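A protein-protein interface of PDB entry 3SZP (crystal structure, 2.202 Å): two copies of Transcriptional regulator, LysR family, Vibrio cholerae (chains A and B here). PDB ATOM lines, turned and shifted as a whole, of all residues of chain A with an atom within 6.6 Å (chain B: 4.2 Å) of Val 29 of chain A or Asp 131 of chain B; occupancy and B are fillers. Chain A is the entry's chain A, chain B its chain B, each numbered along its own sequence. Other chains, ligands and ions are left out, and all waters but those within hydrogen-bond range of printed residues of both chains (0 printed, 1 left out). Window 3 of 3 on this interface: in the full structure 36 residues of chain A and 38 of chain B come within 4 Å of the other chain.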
ATOM      1  N   TYR A  18     -18.230  30.338   4.330  1.00  0.00           N
ATOM      2  CA  TYR A  18     -18.245  29.629   5.604  1.00  0.00           C
ATOM      3  C   TYR A  18     -16.840  29.510   6.169  1.00  0.00           C
ATOM      4  O   TYR A  18     -16.639  29.673   7.369  1.00  0.00           O
ATOM      5  CB  TYR A  18     -18.848  28.233   5.463  1.00  0.00           C
ATOM      6  CG  TYR A  18     -20.354  28.179   5.317  1.00  0.00           C
ATOM      7  CD1 TYR A  18     -21.133  29.309   5.465  1.00  0.00           C
ATOM      8  CD2 TYR A  18     -20.994  26.978   5.034  1.00  0.00           C
ATOM      9  CE1 TYR A  18     -22.512  29.245   5.328  1.00  0.00           C
ATOM     10  CE2 TYR A  18     -22.365  26.901   4.893  1.00  0.00           C
ATOM     11  CZ  TYR A  18     -23.124  28.036   5.039  1.00  0.00           C
ATOM     12  OH  TYR A  18     -24.500  27.965   4.897  1.00  0.00           O
ATOM     13  N   THR A  19     -15.875  29.201   5.303  1.00  0.00           N
ATOM     14  CA  THR A  19     -14.478  29.076   5.706  1.00  0.00           C
ATOM     15  C   THR A  19     -13.957  30.411   6.244  1.00  0.00           C
ATOM     16  O   THR A  19     -13.296  30.466   7.279  1.00  0.00           O
ATOM     17  CB  THR A  19     -13.575  28.592   4.537  1.00  0.00           C
ATOM     18  OG1 THR A  19     -13.758  27.179   4.318  1.00  0.00           O
ATOM     19  CG2 THR A  19     -12.100  28.864   4.838  1.00  0.00           C
ATOM     20  N   SER A  20     -14.255  31.485   5.531  1.00  0.00           N
ATOM     21  CA  SER A  20     -13.856  32.807   5.969  1.00  0.00           C
ATOM     22  C   SER A  20     -14.479  33.094   7.332  1.00  0.00           C
ATOM     23  O   SER A  20     -13.831  33.609   8.236  1.00  0.00           O
ATOM     24  CB  SER A  20     -14.307  33.856   4.957  1.00  0.00           C
ATOM     25  OG  SER A  20     -14.182  35.156   5.509  1.00  0.00           O
ATOM     26  N   SER A  22     -15.609  30.803   9.490  1.00  0.00           N
ATOM     27  CA  SER A  22     -15.053  29.832  10.410  1.00  0.00           C
ATOM     28  C   SER A  22     -13.752  30.375  11.001  1.00  0.00           C
ATOM     29  O   SER A  22     -13.524  30.306  12.215  1.00  0.00           O
ATOM     30  CB  SER A  22     -14.797  28.526   9.659  1.00  0.00           C
ATOM     31  OG  SER A  22     -14.166  27.541  10.461  1.00  0.00           O
ATOM     32  N   LYS A  23     -12.910  30.928  10.132  1.00  0.00           N
ATOM     33  CA  LYS A  23     -11.646  31.522  10.544  1.00  0.00           C
ATOM     34  C   LYS A  23     -11.826  32.591  11.624  1.00  0.00           C
ATOM     35  O   LYS A  23     -11.168  32.550  12.662  1.00  0.00           O
ATOM     36  CB  LYS A  23     -10.917  32.115   9.334  1.00  0.00           C
ATOM     37  CG  LYS A  23     -10.161  31.096   8.472  1.00  0.00           C
ATOM     38  CD  LYS A  23     -10.305  31.425   6.993  1.00  0.00           C
ATOM     39  CE  LYS A  23      -9.034  31.146   6.211  1.00  0.00           C
ATOM     40  NZ  LYS A  23      -8.633  29.709   6.215  1.00  0.00           N
ATOM     41  N   ILE A  27     -15.607  28.858  14.670  1.00  0.00           N
ATOM     42  CA  ILE A  27     -16.668  27.859  14.542  1.00  0.00           C
ATOM     43  C   ILE A  27     -16.357  26.989  13.335  1.00  0.00           C
ATOM     44  O   ILE A  27     -16.223  27.513  12.236  1.00  0.00           O
ATOM     45  CB  ILE A  27     -18.062  28.499  14.321  1.00  0.00           C
ATOM     46  CG1 ILE A  27     -18.361  29.546  15.409  1.00  0.00           C
ATOM     47  CG2 ILE A  27     -19.112  27.415  14.323  1.00  0.00           C
ATOM     48  CD1 ILE A  27     -19.737  30.256  15.283  1.00  0.00           C
ATOM     49  N   PRO A  28     -16.234  25.660  13.528  1.00  0.00           N
ATOM     50  CA  PRO A  28     -15.963  24.802  12.362  1.00  0.00           C
ATOM     51  C   PRO A  28     -17.018  24.998  11.286  1.00  0.00           C
ATOM     52  O   PRO A  28     -18.191  25.264  11.593  1.00  0.00           O
ATOM     53  CB  PRO A  28     -16.055  23.377  12.930  1.00  0.00           C
ATOM     54  CG  PRO A  28     -15.730  23.555  14.397  1.00  0.00           C
ATOM     55  CD  PRO A  28     -16.330  24.885  14.775  1.00  0.00           C
ATOM     56  N   VAL A  29     -16.592  24.859  10.036  1.00  0.00           N
ATOM     57  CA  VAL A  29     -17.503  24.948   8.903  1.00  0.00           C
ATOM     58  C   VAL A  29     -18.704  24.024   9.085  1.00  0.00           C
ATOM     59  O   VAL A  29     -19.833  24.443   8.893  1.00  0.00           O
ATOM     60  CB  VAL A  29     -16.778  24.658   7.574  1.00  0.00           C
ATOM     61  CG1 VAL A  29     -17.781  24.457   6.440  1.00  0.00           C
ATOM     62  CG2 VAL A  29     -15.802  25.798   7.263  1.00  0.00           C
ATOM     63  N   ALA A  30     -18.464  22.777   9.474  1.00  0.00           N
ATOM     64  CA  ALA A  30     -19.565  21.817   9.607  1.00  0.00           C
ATOM     65  C   ALA A  30     -20.624  22.326  10.582  1.00  0.00           C
ATOM     66  O   ALA A  30     -21.824  22.160  10.360  1.00  0.00           O
ATOM     67  CB  ALA A  30     -19.044  20.438  10.035  1.00  0.00           C
ATOM     68  N   THR A  31     -20.177  22.948  11.668  1.00  0.00           N
ATOM     69  CA  THR A  31     -21.106  23.500  12.648  1.00  0.00           C
ATOM     70  C   THR A  31     -21.837  24.749  12.113  1.00  0.00           C
ATOM     71  O   THR A  31     -23.025  24.941  12.368  1.00  0.00           O
ATOM     72  CB  THR A  31     -20.389  23.791  13.996  1.00  0.00           C
ATOM     73  OG1 THR A  31     -19.924  22.551  14.554  1.00  0.00           O
ATOM     74  CG2 THR A  31     -21.325  24.482  14.985  1.00  0.00           C
ATOM     75  N   ILE A  32     -21.119  25.586  11.364  1.00  0.00           N
ATOM     76  CA  ILE A  32     -21.737  26.717  10.679  1.00  0.00           C
ATOM     77  C   ILE A  32     -22.825  26.242   9.718  1.00  0.00           C
ATOM     78  O   ILE A  32     -23.914  26.816   9.668  1.00  0.00           O
ATOM     79  CB  ILE A  32     -20.725  27.558   9.867  1.00  0.00           C
ATOM     80  CG1 ILE A  32     -19.720  28.246  10.791  1.00  0.00           C
ATOM     81  CG2 ILE A  32     -21.475  28.596   8.983  1.00  0.00           C
ATOM     82  CD1 ILE A  32     -18.705  29.138  10.041  1.00  0.00           C
ATOM     83  N   THR A  33     -22.520  25.205   8.948  1.00  0.00           N
ATOM     84  CA  THR A  33     -23.471  24.658   8.005  1.00  0.00           C
ATOM     85  C   THR A  33     -24.710  24.156   8.719  1.00  0.00           C
ATOM     86  O   THR A  33     -25.836  24.360   8.263  1.00  0.00           O
ATOM     87  CB  THR A  33     -22.862  23.482   7.243  1.00  0.00           C
ATOM     88  OG1 THR A  33     -21.800  23.961   6.414  1.00  0.00           O
ATOM     89  CG2 THR A  33     -23.921  22.824   6.356  1.00  0.00           C
ATOM     90  N   ARG A  34     -24.483  23.485   9.836  1.00  0.00           N
ATOM     91  CA  ARG A  34     -25.549  22.886  10.610  1.00  0.00           C
ATOM     92  C   ARG A  34     -26.462  23.962  11.168  1.00  0.00           C
ATOM     93  O   ARG A  34     -27.680  23.810  11.188  1.00  0.00           O
ATOM     94  CB  ARG A  34     -24.938  22.086  11.758  1.00  0.00           C
ATOM     95  CG  ARG A  34     -25.859  21.088  12.426  1.00  0.00           C
ATOM     96  CD  ARG A  34     -25.025  20.009  13.157  1.00  0.00           C
ATOM     97  NE  ARG A  34     -24.212  20.556  14.250  1.00  0.00           N
ATOM     98  CZ  ARG A  34     -22.930  20.255  14.457  1.00  0.00           C
ATOM     99  NH1 ARG A  34     -22.294  19.412  13.636  1.00  0.00           N
ATOM    100  NH2 ARG A  34     -22.276  20.785  15.488  1.00  0.00           N
ATOM    101  N   ALA A  52     -20.658  26.152  -6.227  1.00  0.00           N
ATOM    102  CA  ALA A  52     -19.201  26.243  -6.340  1.00  0.00           C
ATOM    103  C   ALA A  52     -18.569  26.684  -5.029  1.00  0.00           C
ATOM    104  O   ALA A  52     -18.705  26.022  -3.997  1.00  0.00           O
ATOM    105  CB  ALA A  52     -18.816  27.206  -7.452  1.00  0.00           C
ATOM    106  N   ARG A  53     -17.869  27.811  -5.088  1.00  0.00           N
ATOM    107  CA  ARG A  53     -17.317  28.448  -3.902  1.00  0.00           C
ATOM    108  C   ARG A  53     -18.198  29.652  -3.582  1.00  0.00           C
ATOM    109  O   ARG A  53     -18.108  30.244  -2.500  1.00  0.00           O
ATOM    110  CB  ARG A  53     -15.887  28.899  -4.189  1.00  0.00           C
ATOM    111  CG  ARG A  53     -15.014  29.095  -2.961  1.00  0.00           C
ATOM    112  CD  ARG A  53     -13.612  28.544  -3.207  1.00  0.00           C
ATOM    113  NE  ARG A  53     -13.634  27.090  -3.336  1.00  0.00           N
ATOM    114  CZ  ARG A  53     -13.698  26.441  -4.491  1.00  0.00           C
ATOM    115  NH1 ARG A  53     -13.731  27.112  -5.634  1.00  0.00           N
ATOM    116  NH2 ARG A  53     -13.723  25.118  -4.500  1.00  0.00           N
ATOM    117  N   GLN B 129      -9.338  24.602   7.683  1.00  0.00           N
ATOM    118  CA  GLN B 129     -10.548  24.243   6.928  1.00  0.00           C
ATOM    119  C   GLN B 129     -10.269  23.785   5.491  1.00  0.00           C
ATOM    120  O   GLN B 129      -9.469  24.391   4.776  1.00  0.00           O
ATOM    121  CB  GLN B 129     -11.536  25.418   6.883  1.00  0.00           C
ATOM    122  CG  GLN B 129     -11.848  26.069   8.241  1.00  0.00           C
ATOM    123  CD  GLN B 129     -10.847  27.155   8.614  1.00  0.00           C
ATOM    124  OE1 GLN B 129      -9.878  27.405   7.883  1.00  0.00           O
ATOM    125  NE2 GLN B 129     -11.071  27.801   9.753  1.00  0.00           N
ATOM    126  N   ALA B 130     -10.953  22.728   5.061  1.00  0.00           N
ATOM    127  CA  ALA B 130     -10.782  22.206   3.704  1.00  0.00           C
ATOM    128  C   ALA B 130     -11.981  22.505   2.796  1.00  0.00           C
ATOM    129  O   ALA B 130     -11.922  22.271   1.592  1.00  0.00           O
ATOM    130  CB  ALA B 130     -10.485  20.695   3.728  1.00  0.00           C
ATOM    131  N   ASP B 131     -13.047  23.040   3.380  1.00  0.00           N
ATOM    132  CA  ASP B 131     -14.329  23.178   2.700  1.00  0.00           C
ATOM    133  C   ASP B 131     -14.348  24.194   1.560  1.00  0.00           C
ATOM    134  O   ASP B 131     -15.234  24.158   0.711  1.00  0.00           O
ATOM    135  CB  ASP B 131     -15.409  23.541   3.718  1.00  0.00           C
ATOM    136  CG  ASP B 131     -15.368  22.648   4.949  1.00  0.00           C
ATOM    137  OD1 ASP B 131     -16.262  21.772   5.072  1.00  0.00           O
ATOM    138  OD2 ASP B 131     -14.445  22.825   5.786  1.00  0.00           O
ATOM    139  N   ASP B 132     -13.382  25.104   1.544  1.00  0.00           N
ATOM    140  CA  ASP B 132     -13.340  26.138   0.518  1.00  0.00           C
ATOM    141  C   ASP B 132     -12.165  25.957  -0.436  1.00  0.00           C
ATOM    142  O   ASP B 132     -11.822  26.872  -1.187  1.00  0.00           O
ATOM    143  CB  ASP B 132     -13.281  27.529   1.147  1.00  0.00           C
ATOM    144  N   LEU B 133     -11.547  24.783  -0.401  1.00  0.00           N
ATOM    145  CA  LEU B 133     -10.446  24.494  -1.315  1.00  0.00           C
ATOM    146  C   LEU B 133     -10.994  24.263  -2.725  1.00  0.00           C
ATOM    147  O   LEU B 133     -11.935  23.493  -2.919  1.00  0.00           O
ATOM    148  CB  LEU B 133      -9.658  23.265  -0.856  1.00  0.00           C
ATOM    149  CG  LEU B 133      -9.008  23.242   0.530  1.00  0.00           C
ATOM    150  CD1 LEU B 133      -8.152  21.969   0.713  1.00  0.00           C
ATOM    151  CD2 LEU B 133      -8.158  24.477   0.751  1.00  0.00           C
ATOM    152  N   ARG B 143      -8.474  15.570   4.971  1.00  0.00           N
ATOM    153  CA  ARG B 143      -9.370  16.383   5.787  1.00  0.00           C
ATOM    154  C   ARG B 143     -10.000  15.599   6.911  1.00  0.00           C
ATOM    155  O   ARG B 143     -10.002  14.375   6.897  1.00  0.00           O
ATOM    156  CB  ARG B 143     -10.460  17.038   4.938  1.00  0.00           C
ATOM    157  CG  ARG B 143     -11.344  16.071   4.185  1.00  0.00           C
ATOM    158  CD  ARG B 143     -12.652  16.758   3.765  1.00  0.00           C
ATOM    159  NE  ARG B 143     -13.418  17.173   4.935  1.00  0.00           N
ATOM    160  CZ  ARG B 143     -14.087  18.316   5.041  1.00  0.00           C
ATOM    161  NH1 ARG B 143     -14.104  19.185   4.031  1.00  0.00           N
ATOM    162  NH2 ARG B 143     -14.742  18.593   6.163  1.00  0.00           N
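Hydrophobic or aromatic side chains of chain A within 4 Å of the printed part of chain B: Val 29.
Of the 6 printed residues of chain B, 4 touch a printed residue of chain A.
Among the printed residues, no Asp or Glu carboxylate lies within 4 Å of a Lys or Arg side-chain nitrogen of the other chain.
NE of Arg 53 of chain A sits at hydrogen-bond distance from O of Asp 132 of chain B, 2.8 Å away.
N of Asp 132 of chain B sits close to OG1 of Thr 19 of chain A, 3.5 Å away.
The guanidinium group (NH2) of Arg 53 of chain A lies within hydrogen-bond range of the backbone carbonyl oxygen (O) of Leu 133 of chain B (2.9 Å).
NZ of Lys 23 of chain A sits at hydrogen-bond distance from OE1 of Gln 129 of chain B, at 3.1 Å.
The side-chain hydroxyl (OG) of Ser 22 of chain A is in hydrogen-bond range of the side-chain amide nitrogen (NE2) of Gln 129 of chain B, 3.2 Å away.
Printed residues of chain A within 4 Å of Asp 131 of chain B: Val 29 (3.4 Å).
Printed residues of chain B within 4 Å of Lys 23 of chain A: Gln 129 (3.1 Å).
Printed residues of chain A within 4 Å of Asp 132 of chain B: Thr 19 (3.2 Å) and Arg 53 (2.8 Å).
Of the printed residues of chain B, Thr 19 of chain A touches Gln 129 and Asp 132.
Printed residues of chain B within 4 Å of Ser 22 of chain A: Gln 129.
Of the printed residues of chain B, Arg 53 of chain A touches Asp 132 and Leu 133.
Ser 20 of chain A touches none of the printed residues of chain B.
Arg 143 of chain B touches none of the printed residues of chain A.
The nearest printed residue of chain B that does not touch Lys 23 of chain A is Asp 132 of chain B (7.2 Å).
No position is printed for both chains.
Of the 7 pairs that touch across the chains among the printed residues, none has its exchanged pair printed and touching as well.
OG1 of Thr 19 of chain A touches CB of Gln 129 of chain B (3.8 Å).
Val 29 of chain A touches Asp 131 of chain B (CG1 to CG, 3.4 Å).
The side-chain hydroxyl (OG1) of Thr 33 of chain A sits at hydrogen-bond distance from the backbone carbonyl oxygen (O) of Val 29 of chain A, at 3.2 Å.
The backbone carbonyl oxygen (O) of Ile 27 of chain A is in hydrogen-bond range of the side-chain hydroxyl (OG) of Ser 22 of chain A.
NH1 of Arg 143 of chain B is in salt-bridge range of OD1 of Asp 131 of chain B, 3.5 Å away.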
